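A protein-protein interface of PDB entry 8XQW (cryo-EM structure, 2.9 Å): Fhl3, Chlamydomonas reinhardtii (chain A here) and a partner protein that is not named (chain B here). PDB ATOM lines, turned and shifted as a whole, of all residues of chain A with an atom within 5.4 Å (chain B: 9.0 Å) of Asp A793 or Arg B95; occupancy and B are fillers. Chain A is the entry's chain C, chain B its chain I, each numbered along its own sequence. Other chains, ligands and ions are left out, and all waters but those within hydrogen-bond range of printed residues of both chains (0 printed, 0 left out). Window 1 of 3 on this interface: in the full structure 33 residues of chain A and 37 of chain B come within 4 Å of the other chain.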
ATOM      1  N   GLY A 784      20.041   5.349  -6.487  1.00  0.00           N
ATOM      2  CA  GLY A 784      21.010   4.279  -6.470  1.00  0.00           C
ATOM      3  C   GLY A 784      20.514   2.868  -6.684  1.00  0.00           C
ATOM      4  O   GLY A 784      21.044   1.952  -6.058  1.00  0.00           O
ATOM      5  N   GLY A 785      19.499   2.656  -7.511  1.00  0.00           N
ATOM      6  CA  GLY A 785      19.074   1.288  -7.731  1.00  0.00           C
ATOM      7  C   GLY A 785      18.574   0.934  -9.114  1.00  0.00           C
ATOM      8  O   GLY A 785      17.835  -0.038  -9.260  1.00  0.00           O
ATOM      9  N   GLU A 786      18.959   1.692 -10.134  1.00  0.00           N
ATOM     10  CA  GLU A 786      18.331   1.567 -11.440  1.00  0.00           C
ATOM     11  C   GLU A 786      19.049   0.623 -12.389  1.00  0.00           C
ATOM     12  O   GLU A 786      18.476   0.267 -13.421  1.00  0.00           O
ATOM     13  CB  GLU A 786      18.213   2.939 -12.104  1.00  0.00           C
ATOM     14  CG  GLU A 786      17.967   4.063 -11.134  1.00  0.00           C
ATOM     15  CD  GLU A 786      17.854   5.398 -11.825  1.00  0.00           C
ATOM     16  OE1 GLU A 786      16.968   6.195 -11.454  1.00  0.00           O
ATOM     17  OE2 GLU A 786      18.650   5.653 -12.747  1.00  0.00           O
ATOM     18  N   GLY A 787      20.279   0.221 -12.087  1.00  0.00           N
ATOM     19  CA  GLY A 787      21.003  -0.682 -12.950  1.00  0.00           C
ATOM     20  C   GLY A 787      22.007  -0.045 -13.878  1.00  0.00           C
ATOM     21  O   GLY A 787      23.062  -0.638 -14.119  1.00  0.00           O
ATOM     22  N   VAL A 788      21.729   1.151 -14.390  1.00  0.00           N
ATOM     23  CA  VAL A 788      22.581   1.796 -15.378  1.00  0.00           C
ATOM     24  C   VAL A 788      23.904   2.164 -14.732  1.00  0.00           C
ATOM     25  O   VAL A 788      24.071   2.023 -13.521  1.00  0.00           O
ATOM     26  CB  VAL A 788      21.892   3.024 -15.986  1.00  0.00           C
ATOM     27  CG1 VAL A 788      20.762   2.588 -16.865  1.00  0.00           C
ATOM     28  CG2 VAL A 788      21.374   3.919 -14.901  1.00  0.00           C
ATOM     29  N   SER A 791      24.335   4.250 -11.343  1.00  0.00           N
ATOM     30  CA  SER A 791      23.693   3.840 -10.099  1.00  0.00           C
ATOM     31  C   SER A 791      23.753   2.335  -9.916  1.00  0.00           C
ATOM     32  O   SER A 791      23.105   1.604 -10.675  1.00  0.00           O
ATOM     33  CB  SER A 791      22.242   4.304 -10.095  1.00  0.00           C
ATOM     34  OG  SER A 791      21.627   3.996 -11.326  1.00  0.00           O
ATOM     35  N   PRO A 792      24.463   1.825  -8.917  1.00  0.00           N
ATOM     36  CA  PRO A 792      24.574   0.377  -8.737  1.00  0.00           C
ATOM     37  C   PRO A 792      23.276  -0.236  -8.247  1.00  0.00           C
ATOM     38  O   PRO A 792      22.360   0.446  -7.797  1.00  0.00           O
ATOM     39  CB  PRO A 792      25.682   0.233  -7.694  1.00  0.00           C
ATOM     40  CG  PRO A 792      26.330   1.542  -7.631  1.00  0.00           C
ATOM     41  CD  PRO A 792      25.288   2.545  -7.950  1.00  0.00           C
ATOM     42  N   ASP A 793      23.200  -1.559  -8.344  1.00  0.00           N
ATOM     43  CA  ASP A 793      21.962  -2.277  -8.071  1.00  0.00           C
ATOM     44  C   ASP A 793      21.721  -2.520  -6.584  1.00  0.00           C
ATOM     45  O   ASP A 793      20.672  -2.113  -6.073  1.00  0.00           O
ATOM     46  CB  ASP A 793      21.947  -3.599  -8.829  1.00  0.00           C
ATOM     47  CG  ASP A 793      22.288  -3.425 -10.277  1.00  0.00           C
ATOM     48  OD1 ASP A 793      21.974  -2.348 -10.804  1.00  0.00           O
ATOM     49  OD2 ASP A 793      22.879  -4.340 -10.886  1.00  0.00           O
ATOM     50  N   PRO A 794      22.623  -3.175  -5.853  1.00  0.00           N
ATOM     51  CA  PRO A 794      22.332  -3.494  -4.444  1.00  0.00           C
ATOM     52  C   PRO A 794      22.905  -2.525  -3.417  1.00  0.00           C
ATOM     53  O   PRO A 794      22.854  -2.854  -2.228  1.00  0.00           O
ATOM     54  CB  PRO A 794      22.978  -4.876  -4.287  1.00  0.00           C
ATOM     55  CG  PRO A 794      23.676  -5.164  -5.590  1.00  0.00           C
ATOM     56  CD  PRO A 794      23.855  -3.857  -6.251  1.00  0.00           C
ATOM     57  N   ILE A 795      23.428  -1.368  -3.819  1.00  0.00           N
ATOM     58  CA  ILE A 795      23.910  -0.361  -2.871  1.00  0.00           C
ATOM     59  C   ILE A 795      24.953  -0.950  -1.929  1.00  0.00           C
ATOM     60  O   ILE A 795      24.594  -1.460  -0.860  1.00  0.00           O
ATOM     61  CB  ILE A 795      22.759   0.276  -2.083  1.00  0.00           C
ATOM     62  CG1 ILE A 795      21.781   0.936  -3.045  1.00  0.00           C
ATOM     63  CG2 ILE A 795      23.296   1.316  -1.136  1.00  0.00           C
ATOM     64  CD1 ILE A 795      21.006   2.072  -2.445  1.00  0.00           C
ATOM     65  N   ARG B  89      32.836  -3.689 -12.961  1.00  0.00           N
ATOM     66  CA  ARG B  89      31.895  -4.333 -12.060  1.00  0.00           C
ATOM     67  C   ARG B  89      31.605  -3.509 -10.822  1.00  0.00           C
ATOM     68  O   ARG B  89      30.975  -4.019  -9.896  1.00  0.00           O
ATOM     69  CB  ARG B  89      32.404  -5.704 -11.634  1.00  0.00           C
ATOM     70  CG  ARG B  89      32.407  -6.726 -12.731  1.00  0.00           C
ATOM     71  CD  ARG B  89      32.769  -8.078 -12.188  1.00  0.00           C
ATOM     72  NE  ARG B  89      33.277  -8.953 -13.232  1.00  0.00           N
ATOM     73  CZ  ARG B  89      34.547  -8.982 -13.610  1.00  0.00           C
ATOM     74  NH1 ARG B  89      35.425  -8.181 -13.030  1.00  0.00           N
ATOM     75  NH2 ARG B  89      34.942  -9.806 -14.568  1.00  0.00           N
ATOM     76  N   ASP B  90      32.068  -2.266 -10.764  1.00  0.00           N
ATOM     77  CA  ASP B  90      31.731  -1.373  -9.669  1.00  0.00           C
ATOM     78  C   ASP B  90      30.949  -0.160 -10.126  1.00  0.00           C
ATOM     79  O   ASP B  90      30.150   0.374  -9.356  1.00  0.00           O
ATOM     80  CB  ASP B  90      32.995  -0.906  -8.954  1.00  0.00           C
ATOM     81  CG  ASP B  90      33.420  -1.855  -7.865  1.00  0.00           C
ATOM     82  OD1 ASP B  90      32.814  -2.938  -7.757  1.00  0.00           O
ATOM     83  OD2 ASP B  90      34.354  -1.518  -7.110  1.00  0.00           O
ATOM     84  N   ILE B  91      31.176   0.295 -11.354  1.00  0.00           N
ATOM     85  CA  ILE B  91      30.314   1.313 -11.939  1.00  0.00           C
ATOM     86  C   ILE B  91      28.875   0.816 -11.982  1.00  0.00           C
ATOM     87  O   ILE B  91      27.978   1.401 -11.373  1.00  0.00           O
ATOM     88  CB  ILE B  91      30.820   1.696 -13.336  1.00  0.00           C
ATOM     89  CG1 ILE B  91      31.964   2.684 -13.227  1.00  0.00           C
ATOM     90  CG2 ILE B  91      29.739   2.317 -14.142  1.00  0.00           C
ATOM     91  CD1 ILE B  91      32.574   2.998 -14.560  1.00  0.00           C
ATOM     92  N   ILE B  92      28.639  -0.287 -12.689  1.00  0.00           N
ATOM     93  CA  ILE B  92      27.329  -0.918 -12.669  1.00  0.00           C
ATOM     94  C   ILE B  92      27.201  -1.770 -11.417  1.00  0.00           C
ATOM     95  O   ILE B  92      28.168  -2.028 -10.705  1.00  0.00           O
ATOM     96  CB  ILE B  92      27.098  -1.756 -13.933  1.00  0.00           C
ATOM     97  CG1 ILE B  92      27.982  -2.988 -13.900  1.00  0.00           C
ATOM     98  CG2 ILE B  92      27.409  -0.947 -15.157  1.00  0.00           C
ATOM     99  CD1 ILE B  92      28.210  -3.586 -15.239  1.00  0.00           C
ATOM    100  N   GLY B  93      25.996  -2.214 -11.147  1.00  0.00           N
ATOM    101  CA  GLY B  93      25.729  -2.933  -9.924  1.00  0.00           C
ATOM    102  C   GLY B  93      26.434  -4.267  -9.855  1.00  0.00           C
ATOM    103  O   GLY B  93      27.256  -4.619 -10.702  1.00  0.00           O
ATOM    104  N   ASP B  94      26.115  -5.013  -8.807  1.00  0.00           N
ATOM    105  CA  ASP B  94      26.510  -6.405  -8.704  1.00  0.00           C
ATOM    106  C   ASP B  94      25.391  -7.339  -9.132  1.00  0.00           C
ATOM    107  O   ASP B  94      25.519  -8.552  -8.982  1.00  0.00           O
ATOM    108  CB  ASP B  94      26.941  -6.721  -7.270  1.00  0.00           C
ATOM    109  CG  ASP B  94      27.638  -8.057  -7.151  1.00  0.00           C
ATOM    110  OD1 ASP B  94      28.101  -8.577  -8.186  1.00  0.00           O
ATOM    111  OD2 ASP B  94      27.733  -8.584  -6.022  1.00  0.00           O
ATOM    112  N   ARG B  95      24.298  -6.798  -9.649  1.00  0.00           N
ATOM    113  CA  ARG B  95      23.222  -7.588 -10.218  1.00  0.00           C
ATOM    114  C   ARG B  95      23.240  -7.578 -11.731  1.00  0.00           C
ATOM    115  O   ARG B  95      23.057  -8.623 -12.350  1.00  0.00           O
ATOM    116  CB  ARG B  95      21.876  -7.072  -9.721  1.00  0.00           C
ATOM    117  CG  ARG B  95      20.695  -7.747 -10.343  1.00  0.00           C
ATOM    118  CD  ARG B  95      19.402  -7.220  -9.769  1.00  0.00           C
ATOM    119  NE  ARG B  95      19.190  -5.812 -10.080  1.00  0.00           N
ATOM    120  CZ  ARG B  95      18.899  -5.344 -11.290  1.00  0.00           C
ATOM    121  NH1 ARG B  95      18.787  -6.172 -12.319  1.00  0.00           N
ATOM    122  NH2 ARG B  95      18.719  -4.044 -11.475  1.00  0.00           N
ATOM    123  N   MET B  96      23.463  -6.423 -12.349  1.00  0.00           N
ATOM    124  CA  MET B  96      23.611  -6.380 -13.793  1.00  0.00           C
ATOM    125  C   MET B  96      24.917  -7.009 -14.250  1.00  0.00           C
ATOM    126  O   MET B  96      25.015  -7.450 -15.399  1.00  0.00           O
ATOM    127  CB  MET B  96      23.510  -4.942 -14.276  1.00  0.00           C
ATOM    128  CG  MET B  96      23.384  -4.795 -15.767  1.00  0.00           C
ATOM    129  SD  MET B  96      21.761  -5.202 -16.407  1.00  0.00           S
ATOM    130  CE  MET B  96      20.731  -4.601 -15.080  1.00  0.00           C
ATOM    131  N   SER B  97      25.912  -7.090 -13.373  1.00  0.00           N
ATOM    132  CA  SER B  97      27.137  -7.800 -13.711  1.00  0.00           C
ATOM    133  C   SER B  97      26.879  -9.283 -13.909  1.00  0.00           C
ATOM    134  O   SER B  97      27.445  -9.905 -14.814  1.00  0.00           O
ATOM    135  CB  SER B  97      28.174  -7.587 -12.623  1.00  0.00           C
ATOM    136  OG  SER B  97      28.848  -6.371 -12.833  1.00  0.00           O
ATOM    137  N   ARG B  98      26.026  -9.872 -13.076  1.00  0.00           N
ATOM    138  CA  ARG B  98      25.691 -11.280 -13.239  1.00  0.00           C
ATOM    139  C   ARG B  98      24.974 -11.531 -14.554  1.00  0.00           C
ATOM    140  O   ARG B  98      25.294 -12.486 -15.272  1.00  0.00           O
ATOM    141  CB  ARG B  98      24.831 -11.739 -12.074  1.00  0.00           C
ATOM    142  CG  ARG B  98      25.407 -11.381 -10.742  1.00  0.00           C
ATOM    143  CD  ARG B  98      26.540 -12.302 -10.407  1.00  0.00           C
ATOM    144  NE  ARG B  98      26.073 -13.672 -10.230  1.00  0.00           N
ATOM    145  CZ  ARG B  98      25.836 -14.231  -9.048  1.00  0.00           C
ATOM    146  NH1 ARG B  98      26.024 -13.537  -7.933  1.00  0.00           N
ATOM    147  NH2 ARG B  98      25.412 -15.485  -8.978  1.00  0.00           N
ATOM    148  N   ARG B  99      23.988 -10.700 -14.875  1.00  0.00           N
ATOM    149  CA  ARG B  99      23.297 -10.840 -16.146  1.00  0.00           C
ATOM    150  C   ARG B  99      24.272 -10.753 -17.305  1.00  0.00           C
ATOM    151  O   ARG B  99      24.204 -11.554 -18.244  1.00  0.00           O
ATOM    152  CB  ARG B  99      22.226  -9.767 -16.267  1.00  0.00           C
ATOM    153  CG  ARG B  99      21.410  -9.853 -17.515  1.00  0.00           C
ATOM    154  CD  ARG B  99      20.175 -10.690 -17.286  1.00  0.00           C
ATOM    155  NE  ARG B  99      20.326 -12.043 -17.807  1.00  0.00           N
ATOM    156  CZ  ARG B  99      19.830 -12.450 -18.967  1.00  0.00           C
ATOM    157  NH1 ARG B  99      19.147 -11.609 -19.726  1.00  0.00           N
ATOM    158  NH2 ARG B  99      20.017 -13.695 -19.369  1.00  0.00           N
ATOM    159  N   LEU B 100      25.195  -9.795 -17.252  1.00  0.00           N
ATOM    160  CA  LEU B 100      26.162  -9.639 -18.331  1.00  0.00           C
ATOM    161  C   LEU B 100      27.053 -10.861 -18.468  1.00  0.00           C
ATOM    162  O   LEU B 100      27.335 -11.317 -19.583  1.00  0.00           O
ATOM    163  CB  LEU B 100      27.006  -8.403 -18.081  1.00  0.00           C
ATOM    164  CG  LEU B 100      27.418  -7.672 -19.336  1.00  0.00           C
ATOM    165  CD1 LEU B 100      26.186  -7.379 -20.145  1.00  0.00           C
ATOM    166  CD2 LEU B 100      28.122  -6.404 -18.953  1.00  0.00           C
ATOM    167  N   GLU B 101      27.515 -11.404 -17.347  1.00  0.00           N
ATOM    168  CA  GLU B 101      28.377 -12.573 -17.408  1.00  0.00           C
ATOM    169  C   GLU B 101      27.643 -13.766 -17.997  1.00  0.00           C
ATOM    170  O   GLU B 101      28.207 -14.511 -18.808  1.00  0.00           O
ATOM    171  CB  GLU B 101      28.918 -12.886 -16.022  1.00  0.00           C
ATOM    172  CG  GLU B 101      29.944 -11.872 -15.560  1.00  0.00           C
ATOM    173  CD  GLU B 101      30.393 -12.089 -14.129  1.00  0.00           C
ATOM    174  OE1 GLU B 101      29.631 -12.701 -13.355  1.00  0.00           O
ATOM    175  OE2 GLU B 101      31.506 -11.642 -13.777  1.00  0.00           O
ATOM    176  N   ASP B 102      26.376 -13.952 -17.633  1.00  0.00           N
ATOM    177  CA  ASP B 102      25.636 -15.085 -18.181  1.00  0.00           C
ATOM    178  C   ASP B 102      25.357 -14.913 -19.666  1.00  0.00           C
ATOM    179  O   ASP B 102      25.399 -15.891 -20.423  1.00  0.00           O
ATOM    180  CB  ASP B 102      24.340 -15.296 -17.420  1.00  0.00           C
ATOM    181  CG  ASP B 102      24.560 -15.392 -15.938  1.00  0.00           C
ATOM    182  OD1 ASP B 102      25.651 -15.843 -15.541  1.00  0.00           O
ATOM    183  OD2 ASP B 102      23.652 -15.012 -15.168  1.00  0.00           O
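CA of Pro A792 touches CA of Gly B93 (3.7 Å).
Asp A793 touches Gly B93 (N to CA, 3.3 Å).
OD2 of Asp A793 touches N of Asp B94 (3.9 Å).
Asp B94 touches Pro A794.
The backbone NH of Gly A787 sits close to the side-chain carboxylate of Asp A793 (3.3 Å).
O of Gly A784 sits close to O of Pro A792 (2.7 Å).
The backbone carbonyl oxygen (O) of Gly B93 sits at hydrogen-bond distance from the side-chain hydroxyl (OG) of Ser B97 (3.2 Å).
Of the 14 printed residues of chain B, 4 touch a printed residue of chain A.
Printed residues of chain B that touch a printed residue of chain A: Gly B93, Asp B94, Arg B95 and Met B96.
Hydrophobic or aromatic side chains of chain B within 4 Å of the printed part of chain A: Met B96.
Of the 10 printed residues of chain A, 3 touch a printed residue of chain B.
Along chain A the printed residues that touch a printed residue of chain B span positions 792 to 794.
OD1 of Asp A793 lies within salt-bridge range of NH2 of Arg B95 (3.7 Å).
The backbone NH (N) of Met B96 sits at hydrogen-bond distance from the side-chain carboxylate (OD2) of Asp A793, at 2.6 Å.
Asp A793 touches just these residues of chain B: Gly B93, Asp B94, Arg B95 and Met B96.
Arg B95 touches one residue of chain A.
No residue of chain B comes within 4 Å of Gly A787.
Pro A792 touches just one residue of chain B: Gly B93 (3.7 Å).
Pro A794 touches one residue of chain B.
Of the printed residues of chain A, Gly B93 touches Pro A792 and Asp A793.
Of the printed residues of chain A, Met B96 touches Asp A793 (2.6 Å).
Of the printed residues of chain A, Asp B94 touches Asp A793 and Pro A794.
Ile B92 touches none of the printed residues of chain A.
Glu A786 touches none of the printed residues of chain B.
The nearest residue of chain B that does not touch Asp A793 is Ser B97 (4.8 Å).
The nearest residue of chain A that does not touch Arg B95 is Gly A787 (4.3 Å).
The nearest printed residue of chain A that does not touch Met B96 is Gly A787 (4.3 Å).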
